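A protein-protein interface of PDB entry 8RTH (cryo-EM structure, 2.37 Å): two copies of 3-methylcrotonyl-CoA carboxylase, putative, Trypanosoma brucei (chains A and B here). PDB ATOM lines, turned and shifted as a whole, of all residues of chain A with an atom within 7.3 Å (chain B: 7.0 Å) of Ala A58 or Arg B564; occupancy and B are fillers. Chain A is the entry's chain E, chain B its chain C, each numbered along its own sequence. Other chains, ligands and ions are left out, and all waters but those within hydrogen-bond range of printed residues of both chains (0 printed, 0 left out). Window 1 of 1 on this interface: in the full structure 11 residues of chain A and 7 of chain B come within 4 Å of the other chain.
NH2 of Arg B564 is in hydrogen-bond range of O of Pro A47, 3.3 Å away.
O of Glu A46 lies within hydrogen-bond range of NH1 of Arg B564 (2.4 Å).
O of Leu A53 lies within hydrogen-bond range of NH2 of Arg B556 (3.1 Å).
The backbone carbonyl oxygen (O) of Arg B564 is in hydrogen-bond range of the backbone NH (N) of Ala A58, 2.8 Å away.
The backbone carbonyl oxygen of Phe B565 lies within hydrogen-bond range of the backbone NH of Val B557 (2.9 Å).
OG1 of Thr A38 is in hydrogen-bond range of N of Asp A56, at 2.9 Å.
The backbone NH (N) of Ala A40 sits at hydrogen-bond distance from the backbone carbonyl oxygen (O) of Glu A57 (2.7 Å).
The guanidinium group (NE) of Arg B564 is in salt-bridge range of the side-chain carboxylate (OE2) of Glu B543 (2.9 Å).
N of Phe A59 lies within hydrogen-bond range of O of Ala A40, at 3.1 Å.
The backbone carbonyl oxygen (O) of Arg B556 lies within hydrogen-bond range of the backbone NH (N) of Glu B543, 2.9 Å away.
Arg B564 touches Cys A42.
Val A52 touches Arg B556.
Asp A56 touches Phe B565.
Glu A57 touches Arg B564.
O of Glu B562 touches O of Ala A58, 3.7 Å away.
O of Ala A58 touches CA of Thr B563, at 3.7 Å.
Glu B562 touches Phe A59.
Val A60 touches Gly B561.
Val A60 touches Glu B562.
Ala A58 touches just these residues of chain B: Glu B562 (3.7 Å), Thr B563 (3.7 Å) and Arg B564 (2.8 Å).
Arg B564 touches just these residues of chain A: Cys A42 (3.98 Å), Glu A46 (2.4 Å), Pro A47 (3.3 Å), Glu A57 (3.7 Å) and Ala A58 (2.8 Å).
Printed residues of chain B within 4 Å of Phe A59: Glu B562.
Printed residues of chain B within 4 Å of Cys A42: Arg B564.
Val A41 touches none of the printed residues of chain B.
His A51 touches none of the printed residues of chain B.
The nearest residue of chain B that does not touch Ala A58 is Phe B565 (5.0 Å).
The nearest printed residue of chain A that does not touch Phe B565 is Glu A57 (4.3 Å).
Hydrophobic or aromatic side chains of chain A within 4 Å of the printed part of chain B: Leu A53, Ala A58, Phe A59 and Val A60.
No position is printed for both chains.
Of the 13 pairs that touch across the chains among the printed residues, none has its exchanged pair printed and touching as well.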
ATOM      1  N   THR A  38     -27.303   6.790 -36.170  1.00  0.00           N
ATOM      2  CA  THR A  38     -26.753   5.525 -35.701  1.00  0.00           C
ATOM      3  C   THR A  38     -26.304   5.653 -34.252  1.00  0.00           C
ATOM      4  O   THR A  38     -25.664   6.642 -33.879  1.00  0.00           O
ATOM      5  CB  THR A  38     -25.576   5.087 -36.574  1.00  0.00           C
ATOM      6  OG1 THR A  38     -24.556   6.093 -36.543  1.00  0.00           O
ATOM      7  CG2 THR A  38     -26.029   4.884 -38.009  1.00  0.00           C
ATOM      8  N   VAL A  39     -26.643   4.653 -33.443  1.00  0.00           N
ATOM      9  CA  VAL A  39     -26.227   4.572 -32.049  1.00  0.00           C
ATOM     10  C   VAL A  39     -25.480   3.261 -31.858  1.00  0.00           C
ATOM     11  O   VAL A  39     -25.966   2.201 -32.267  1.00  0.00           O
ATOM     12  CB  VAL A  39     -27.426   4.664 -31.089  1.00  0.00           C
ATOM     13  CG1 VAL A  39     -26.963   4.526 -29.649  1.00  0.00           C
ATOM     14  CG2 VAL A  39     -28.162   5.975 -31.289  1.00  0.00           C
ATOM     15  N   ALA A  40     -24.306   3.332 -31.241  1.00  0.00           N
ATOM     16  CA  ALA A  40     -23.444   2.175 -31.056  1.00  0.00           C
ATOM     17  C   ALA A  40     -23.451   1.725 -29.601  1.00  0.00           C
ATOM     18  O   ALA A  40     -23.922   2.426 -28.702  1.00  0.00           O
ATOM     19  CB  ALA A  40     -22.014   2.482 -31.508  1.00  0.00           C
ATOM     20  N   VAL A  41     -22.913   0.528 -29.384  1.00  0.00           N
ATOM     21  CA  VAL A  41     -22.825  -0.092 -28.069  1.00  0.00           C
ATOM     22  C   VAL A  41     -21.396  -0.576 -27.871  1.00  0.00           C
ATOM     23  O   VAL A  41     -20.816  -1.188 -28.772  1.00  0.00           O
ATOM     24  CB  VAL A  41     -23.825  -1.256 -27.925  1.00  0.00           C
ATOM     25  CG1 VAL A  41     -23.394  -2.207 -26.825  1.00  0.00           C
ATOM     26  CG2 VAL A  41     -25.218  -0.721 -27.652  1.00  0.00           C
ATOM     27  N   CYS A  42     -20.829  -0.296 -26.700  1.00  0.00           N
ATOM     28  CA  CYS A  42     -19.447  -0.665 -26.425  1.00  0.00           C
ATOM     29  C   CYS A  42     -19.263  -0.814 -24.923  1.00  0.00           C
ATOM     30  O   CYS A  42     -20.165  -0.534 -24.133  1.00  0.00           O
ATOM     31  CB  CYS A  42     -18.471   0.369 -26.993  1.00  0.00           C
ATOM     32  SG  CYS A  42     -18.644   2.021 -26.284  1.00  0.00           S
ATOM     33  N   CYS A  43     -18.076  -1.272 -24.542  1.00  0.00           N
ATOM     34  CA  CYS A  43     -17.661  -1.376 -23.154  1.00  0.00           C
ATOM     35  C   CYS A  43     -16.516  -0.402 -22.893  1.00  0.00           C
ATOM     36  O   CYS A  43     -16.009   0.258 -23.803  1.00  0.00           O
ATOM     37  CB  CYS A  43     -17.262  -2.814 -22.815  1.00  0.00           C
ATOM     38  SG  CYS A  43     -15.934  -3.486 -23.835  1.00  0.00           S
ATOM     39  N   GLU A  44     -16.102  -0.321 -21.627  1.00  0.00           N
ATOM     40  CA  GLU A  44     -15.083   0.642 -21.225  1.00  0.00           C
ATOM     41  C   GLU A  44     -13.712   0.350 -21.819  1.00  0.00           C
ATOM     42  O   GLU A  44     -12.836   1.221 -21.760  1.00  0.00           O
ATOM     43  CB  GLU A  44     -14.978   0.690 -19.700  1.00  0.00           C
ATOM     44  CG  GLU A  44     -16.175   1.326 -19.017  1.00  0.00           C
ATOM     45  CD  GLU A  44     -16.046   1.336 -17.508  1.00  0.00           C
ATOM     46  OE1 GLU A  44     -15.014   0.859 -16.994  1.00  0.00           O
ATOM     47  OE2 GLU A  44     -16.979   1.822 -16.835  1.00  0.00           O
ATOM     48  N   GLY A  45     -13.501  -0.833 -22.384  1.00  0.00           N
ATOM     49  CA  GLY A  45     -12.205  -1.181 -22.929  1.00  0.00           C
ATOM     50  C   GLY A  45     -12.108  -1.018 -24.432  1.00  0.00           C
ATOM     51  O   GLY A  45     -11.286  -1.676 -25.078  1.00  0.00           O
ATOM     52  N   GLU A  46     -12.936  -0.144 -25.006  1.00  0.00           N
ATOM     53  CA  GLU A  46     -12.998   0.067 -26.451  1.00  0.00           C
ATOM     54  C   GLU A  46     -12.805   1.550 -26.746  1.00  0.00           C
ATOM     55  O   GLU A  46     -13.767   2.258 -27.077  1.00  0.00           O
ATOM     56  CB  GLU A  46     -14.322  -0.432 -27.027  1.00  0.00           C
ATOM     57  CG  GLU A  46     -14.613  -1.897 -26.757  1.00  0.00           C
ATOM     58  CD  GLU A  46     -13.692  -2.831 -27.518  1.00  0.00           C
ATOM     59  OE1 GLU A  46     -13.039  -2.378 -28.481  1.00  0.00           O
ATOM     60  OE2 GLU A  46     -13.624  -4.022 -27.152  1.00  0.00           O
ATOM     61  N   PRO A  47     -11.573   2.057 -26.642  1.00  0.00           N
ATOM     62  CA  PRO A  47     -11.345   3.477 -26.939  1.00  0.00           C
ATOM     63  C   PRO A  47     -11.231   3.785 -28.420  1.00  0.00           C
ATOM     64  O   PRO A  47     -11.416   4.948 -28.803  1.00  0.00           O
ATOM     65  CB  PRO A  47     -10.027   3.773 -26.215  1.00  0.00           C
ATOM     66  CG  PRO A  47      -9.298   2.477 -26.268  1.00  0.00           C
ATOM     67  CD  PRO A  47     -10.343   1.386 -26.186  1.00  0.00           C
ATOM     68  N   ASN A  48     -10.940   2.793 -29.264  1.00  0.00           N
ATOM     69  CA  ASN A  48     -10.760   3.034 -30.691  1.00  0.00           C
ATOM     70  C   ASN A  48     -11.455   1.975 -31.536  1.00  0.00           C
ATOM     71  O   ASN A  48     -10.967   1.621 -32.616  1.00  0.00           O
ATOM     72  CB  ASN A  48      -9.276   3.092 -31.057  1.00  0.00           C
ATOM     73  CG  ASN A  48      -8.588   4.317 -30.496  1.00  0.00           C
ATOM     74  OD1 ASN A  48      -9.141   5.416 -30.516  1.00  0.00           O
ATOM     75  ND2 ASN A  48      -7.376   4.134 -29.987  1.00  0.00           N
ATOM     76  N   ALA A  49     -12.584   1.453 -31.066  1.00  0.00           N
ATOM     77  CA  ALA A  49     -13.339   0.488 -31.851  1.00  0.00           C
ATOM     78  C   ALA A  49     -13.882   1.147 -33.112  1.00  0.00           C
ATOM     79  O   ALA A  49     -14.351   2.288 -33.082  1.00  0.00           O
ATOM     80  CB  ALA A  49     -14.481  -0.096 -31.024  1.00  0.00           C
ATOM     81  N   HIS A  51     -16.535   0.522 -35.012  1.00  0.00           N
ATOM     82  CA  HIS A  51     -17.964   0.820 -35.035  1.00  0.00           C
ATOM     83  C   HIS A  51     -18.302   2.016 -34.156  1.00  0.00           C
ATOM     84  O   HIS A  51     -19.231   2.769 -34.470  1.00  0.00           O
ATOM     85  CB  HIS A  51     -18.767  -0.405 -34.604  1.00  0.00           C
ATOM     86  CG  HIS A  51     -18.600  -0.761 -33.160  1.00  0.00           C
ATOM     87  ND1 HIS A  51     -17.499  -1.436 -32.683  1.00  0.00           N
ATOM     88  CD2 HIS A  51     -19.400  -0.540 -32.090  1.00  0.00           C
ATOM     89  CE1 HIS A  51     -17.624  -1.613 -31.380  1.00  0.00           C
ATOM     90  NE2 HIS A  51     -18.770  -1.079 -30.996  1.00  0.00           N
ATOM     91  N   VAL A  52     -17.571   2.206 -33.057  1.00  0.00           N
ATOM     92  CA  VAL A  52     -17.790   3.376 -32.215  1.00  0.00           C
ATOM     93  C   VAL A  52     -17.447   4.651 -32.975  1.00  0.00           C
ATOM     94  O   VAL A  52     -18.161   5.657 -32.883  1.00  0.00           O
ATOM     95  CB  VAL A  52     -16.979   3.255 -30.912  1.00  0.00           C
ATOM     96  CG1 VAL A  52     -17.176   4.484 -30.046  1.00  0.00           C
ATOM     97  CG2 VAL A  52     -17.381   2.002 -30.158  1.00  0.00           C
ATOM     98  N   LEU A  53     -16.351   4.631 -33.736  1.00  0.00           N
ATOM     99  CA  LEU A  53     -15.961   5.810 -34.499  1.00  0.00           C
ATOM    100  C   LEU A  53     -16.912   6.077 -35.659  1.00  0.00           C
ATOM    101  O   LEU A  53     -17.135   7.238 -36.018  1.00  0.00           O
ATOM    102  CB  LEU A  53     -14.532   5.652 -35.014  1.00  0.00           C
ATOM    103  CG  LEU A  53     -13.458   5.409 -33.954  1.00  0.00           C
ATOM    104  CD1 LEU A  53     -12.078   5.372 -34.587  1.00  0.00           C
ATOM    105  CD2 LEU A  53     -13.523   6.467 -32.867  1.00  0.00           C
ATOM    106  N   ALA A  55     -20.116   5.590 -35.752  1.00  0.00           N
ATOM    107  CA  ALA A  55     -21.473   5.866 -35.308  1.00  0.00           C
ATOM    108  C   ALA A  55     -21.604   7.304 -34.827  1.00  0.00           C
ATOM    109  O   ALA A  55     -20.635   7.925 -34.386  1.00  0.00           O
ATOM    110  CB  ALA A  55     -21.885   4.910 -34.189  1.00  0.00           C
ATOM    111  N   ASP A  56     -22.826   7.832 -34.928  1.00  0.00           N
ATOM    112  CA  ASP A  56     -23.093   9.179 -34.439  1.00  0.00           C
ATOM    113  C   ASP A  56     -22.953   9.256 -32.924  1.00  0.00           C
ATOM    114  O   ASP A  56     -22.411  10.231 -32.393  1.00  0.00           O
ATOM    115  CB  ASP A  56     -24.488   9.625 -34.872  1.00  0.00           C
ATOM    116  CG  ASP A  56     -24.671   9.578 -36.375  1.00  0.00           C
ATOM    117  OD1 ASP A  56     -23.672   9.751 -37.102  1.00  0.00           O
ATOM    118  OD2 ASP A  56     -25.814   9.364 -36.830  1.00  0.00           O
ATOM    119  N   GLU A  57     -23.437   8.240 -32.213  1.00  0.00           N
ATOM    120  CA  GLU A  57     -23.375   8.208 -30.761  1.00  0.00           C
ATOM    121  C   GLU A  57     -23.048   6.795 -30.303  1.00  0.00           C
ATOM    122  O   GLU A  57     -23.271   5.818 -31.022  1.00  0.00           O
ATOM    123  CB  GLU A  57     -24.690   8.672 -30.124  1.00  0.00           C
ATOM    124  CG  GLU A  57     -25.003  10.140 -30.335  1.00  0.00           C
ATOM    125  CD  GLU A  57     -26.412  10.497 -29.913  1.00  0.00           C
ATOM    126  OE1 GLU A  57     -27.272   9.592 -29.891  1.00  0.00           O
ATOM    127  OE2 GLU A  57     -26.661  11.680 -29.601  1.00  0.00           O
ATOM    128  N   ALA A  58     -22.510   6.697 -29.090  1.00  0.00           N
ATOM    129  CA  ALA A  58     -22.191   5.415 -28.484  1.00  0.00           C
ATOM    130  C   ALA A  58     -22.576   5.446 -27.014  1.00  0.00           C
ATOM    131  O   ALA A  58     -22.603   6.505 -26.383  1.00  0.00           O
ATOM    132  CB  ALA A  58     -20.703   5.071 -28.634  1.00  0.00           C
ATOM    133  N   PHE A  59     -22.880   4.267 -26.476  1.00  0.00           N
ATOM    134  CA  PHE A  59     -23.261   4.110 -25.079  1.00  0.00           C
ATOM    135  C   PHE A  59     -22.449   2.973 -24.480  1.00  0.00           C
ATOM    136  O   PHE A  59     -22.412   1.875 -25.042  1.00  0.00           O
ATOM    137  CB  PHE A  59     -24.760   3.824 -24.951  1.00  0.00           C
ATOM    138  CG  PHE A  59     -25.292   3.967 -23.555  1.00  0.00           C
ATOM    139  CD1 PHE A  59     -25.181   2.932 -22.645  1.00  0.00           C
ATOM    140  CD2 PHE A  59     -25.919   5.133 -23.157  1.00  0.00           C
ATOM    141  CE1 PHE A  59     -25.677   3.060 -21.365  1.00  0.00           C
ATOM    142  CE2 PHE A  59     -26.418   5.268 -21.879  1.00  0.00           C
ATOM    143  CZ  PHE A  59     -26.294   4.230 -20.981  1.00  0.00           C
ATOM    144  N   VAL A  60     -21.805   3.230 -23.347  1.00  0.00           N
ATOM    145  CA  VAL A  60     -20.990   2.209 -22.701  1.00  0.00           C
ATOM    146  C   VAL A  60     -21.889   1.327 -21.844  1.00  0.00           C
ATOM    147  O   VAL A  60     -22.788   1.814 -21.150  1.00  0.00           O
ATOM    148  CB  VAL A  60     -19.857   2.845 -21.876  1.00  0.00           C
ATOM    149  CG1 VAL A  60     -20.395   3.575 -20.668  1.00  0.00           C
ATOM    150  CG2 VAL A  60     -18.855   1.787 -21.454  1.00  0.00           C
ATOM    151  N   ALA A  79     -29.932   2.057 -22.648  1.00  0.00           N
ATOM    152  CA  ALA A  79     -29.161   2.825 -23.619  1.00  0.00           C
ATOM    153  C   ALA A  79     -30.051   3.344 -24.739  1.00  0.00           C
ATOM    154  O   ALA A  79     -29.958   4.512 -25.134  1.00  0.00           O
ATOM    155  CB  ALA A  79     -28.038   1.961 -24.189  1.00  0.00           C
ATOM    156  N   LEU A  83     -30.946   7.475 -25.363  1.00  0.00           N
ATOM    157  CA  LEU A  83     -30.569   8.123 -26.611  1.00  0.00           C
ATOM    158  C   LEU A  83     -31.735   8.261 -27.580  1.00  0.00           C
ATOM    159  O   LEU A  83     -31.513   8.601 -28.746  1.00  0.00           O
ATOM    160  CB  LEU A  83     -29.425   7.362 -27.284  1.00  0.00           C
ATOM    161  CG  LEU A  83     -28.012   7.652 -26.770  1.00  0.00           C
ATOM    162  CD1 LEU A  83     -27.764   9.150 -26.695  1.00  0.00           C
ATOM    163  CD2 LEU A  83     -27.770   7.001 -25.423  1.00  0.00           C
ATOM    164  N   GLU B 543     -11.320  12.375 -24.654  1.00  0.00           N
ATOM    165  CA  GLU B 543     -10.433  11.280 -25.028  1.00  0.00           C
ATOM    166  C   GLU B 543      -9.283  11.774 -25.895  1.00  0.00           C
ATOM    167  O   GLU B 543      -8.120  11.425 -25.659  1.00  0.00           O
ATOM    168  CB  GLU B 543     -11.229  10.199 -25.756  1.00  0.00           C
ATOM    169  CG  GLU B 543     -12.472   9.750 -25.012  1.00  0.00           C
ATOM    170  CD  GLU B 543     -13.400   8.926 -25.878  1.00  0.00           C
ATOM    171  OE1 GLU B 543     -13.084   8.733 -27.071  1.00  0.00           O
ATOM    172  OE2 GLU B 543     -14.445   8.474 -25.369  1.00  0.00           O
ATOM    173  N   ARG B 556     -13.253  14.151 -29.359  1.00  0.00           N
ATOM    174  CA  ARG B 556     -13.957  12.957 -28.916  1.00  0.00           C
ATOM    175  C   ARG B 556     -14.171  13.048 -27.413  1.00  0.00           C
ATOM    176  O   ARG B 556     -13.212  13.240 -26.660  1.00  0.00           O
ATOM    177  CB  ARG B 556     -13.164  11.697 -29.261  1.00  0.00           C
ATOM    178  CG  ARG B 556     -13.208  11.315 -30.724  1.00  0.00           C
ATOM    179  CD  ARG B 556     -14.516  10.628 -31.055  1.00  0.00           C
ATOM    180  NE  ARG B 556     -14.599  10.254 -32.460  1.00  0.00           N
ATOM    181  CZ  ARG B 556     -15.606   9.579 -32.995  1.00  0.00           C
ATOM    182  NH1 ARG B 556     -16.630   9.171 -32.261  1.00  0.00           N
ATOM    183  NH2 ARG B 556     -15.586   9.306 -34.296  1.00  0.00           N
ATOM    184  N   VAL B 557     -15.422  12.919 -26.977  1.00  0.00           N
ATOM    185  CA  VAL B 557     -15.771  13.122 -25.580  1.00  0.00           C
ATOM    186  C   VAL B 557     -16.647  11.980 -25.090  1.00  0.00           C
ATOM    187  O   VAL B 557     -17.299  11.273 -25.865  1.00  0.00           O
ATOM    188  CB  VAL B 557     -16.490  14.467 -25.344  1.00  0.00           C
ATOM    189  CG1 VAL B 557     -15.563  15.629 -25.642  1.00  0.00           C
ATOM    190  CG2 VAL B 557     -17.747  14.547 -26.188  1.00  0.00           C
ATOM    191  N   THR B 558     -16.631  11.809 -23.772  1.00  0.00           N
ATOM    192  CA  THR B 558     -17.555  10.952 -23.041  1.00  0.00           C
ATOM    193  C   THR B 558     -18.279  11.837 -22.036  1.00  0.00           C
ATOM    194  O   THR B 558     -17.682  12.275 -21.046  1.00  0.00           O
ATOM    195  CB  THR B 558     -16.822   9.811 -22.341  1.00  0.00           C
ATOM    196  OG1 THR B 558     -16.083   9.053 -23.304  1.00  0.00           O
ATOM    197  CG2 THR B 558     -17.812   8.900 -21.637  1.00  0.00           C
ATOM    198  N   VAL B 559     -19.540  12.130 -22.311  1.00  0.00           N
ATOM    199  CA  VAL B 559     -20.371  12.920 -21.415  1.00  0.00           C
ATOM    200  C   VAL B 559     -20.902  12.022 -20.310  1.00  0.00           C
ATOM    201  O   VAL B 559     -21.306  10.871 -20.553  1.00  0.00           O
ATOM    202  CB  VAL B 559     -21.513  13.598 -22.192  1.00  0.00           C
ATOM    203  CG1 VAL B 559     -22.403  14.392 -21.252  1.00  0.00           C
ATOM    204  CG2 VAL B 559     -20.944  14.503 -23.267  1.00  0.00           C
ATOM    205  N   GLY B 561     -20.679   9.417 -17.788  1.00  0.00           N
ATOM    206  CA  GLY B 561     -19.764   8.303 -17.891  1.00  0.00           C
ATOM    207  C   GLY B 561     -20.237   7.314 -18.930  1.00  0.00           C
ATOM    208  O   GLY B 561     -19.699   6.210 -19.034  1.00  0.00           O
ATOM    209  N   GLU B 562     -21.248   7.703 -19.709  1.00  0.00           N
ATOM    210  CA  GLU B 562     -21.906   6.750 -20.586  1.00  0.00           C
ATOM    211  C   GLU B 562     -22.281   7.277 -21.965  1.00  0.00           C
ATOM    212  O   GLU B 562     -22.884   6.523 -22.733  1.00  0.00           O
ATOM    213  CB  GLU B 562     -23.174   6.206 -19.907  1.00  0.00           C
ATOM    214  CG  GLU B 562     -24.344   7.182 -19.875  1.00  0.00           C
ATOM    215  CD  GLU B 562     -24.099   8.384 -18.982  1.00  0.00           C
ATOM    216  OE1 GLU B 562     -23.204   8.313 -18.115  1.00  0.00           O
ATOM    217  OE2 GLU B 562     -24.803   9.402 -19.152  1.00  0.00           O
ATOM    218  N   THR B 563     -21.955   8.518 -22.321  1.00  0.00           N
ATOM    219  CA  THR B 563     -22.358   9.034 -23.632  1.00  0.00           C
ATOM    220  C   THR B 563     -21.119   9.402 -24.444  1.00  0.00           C
ATOM    221  O   THR B 563     -20.622  10.522 -24.355  1.00  0.00           O
ATOM    222  CB  THR B 563     -23.296  10.226 -23.483  1.00  0.00           C
ATOM    223  OG1 THR B 563     -24.374   9.876 -22.606  1.00  0.00           O
ATOM    224  CG2 THR B 563     -23.867  10.617 -24.834  1.00  0.00           C
ATOM    225  N   ARG B 564     -20.633   8.470 -25.257  1.00  0.00           N
ATOM    226  CA  ARG B 564     -19.439   8.703 -26.058  1.00  0.00           C
ATOM    227  C   ARG B 564     -19.822   9.182 -27.452  1.00  0.00           C
ATOM    228  O   ARG B 564     -20.675   8.575 -28.108  1.00  0.00           O
ATOM    229  CB  ARG B 564     -18.600   7.433 -26.163  1.00  0.00           C
ATOM    230  CG  ARG B 564     -18.023   6.950 -24.855  1.00  0.00           C
ATOM    231  CD  ARG B 564     -17.070   5.806 -25.106  1.00  0.00           C
ATOM    232  NE  ARG B 564     -16.043   6.177 -26.071  1.00  0.00           N
ATOM    233  CZ  ARG B 564     -15.186   5.326 -26.617  1.00  0.00           C
ATOM    234  NH1 ARG B 564     -15.213   4.037 -26.325  1.00  0.00           N
ATOM    235  NH2 ARG B 564     -14.281   5.780 -27.479  1.00  0.00           N
ATOM    236  N   PHE B 565     -19.187  10.261 -27.902  1.00  0.00           N
ATOM    237  CA  PHE B 565     -19.393  10.745 -29.263  1.00  0.00           C
ATOM    238  C   PHE B 565     -18.303  11.751 -29.598  1.00  0.00           C
ATOM    239  O   PHE B 565     -17.608  12.261 -28.717  1.00  0.00           O
ATOM    240  CB  PHE B 565     -20.780  11.368 -29.447  1.00  0.00           C
ATOM    241  CG  PHE B 565     -21.040  12.553 -28.563  1.00  0.00           C
ATOM    242  CD1 PHE B 565     -20.740  13.833 -28.992  1.00  0.00           C
ATOM    243  CD2 PHE B 565     -21.596  12.387 -27.309  1.00  0.00           C
ATOM    244  CE1 PHE B 565     -20.981  14.921 -28.183  1.00  0.00           C
ATOM    245  CE2 PHE B 565     -21.840  13.470 -26.497  1.00  0.00           C
ATOM    246  CZ  PHE B 565     -21.533  14.739 -26.934  1.00  0.00           C
ATOM    247  N   GLY B 566     -18.172  12.043 -30.887  1.00  0.00           N
ATOM    248  CA  GLY B 566     -17.246  13.053 -31.360  1.00  0.00           C
ATOM    249  C   GLY B 566     -17.993  14.211 -31.991  1.00  0.00           C
ATOM    250  O   GLY B 566     -19.066  14.035 -32.570  1.00  0.00           O
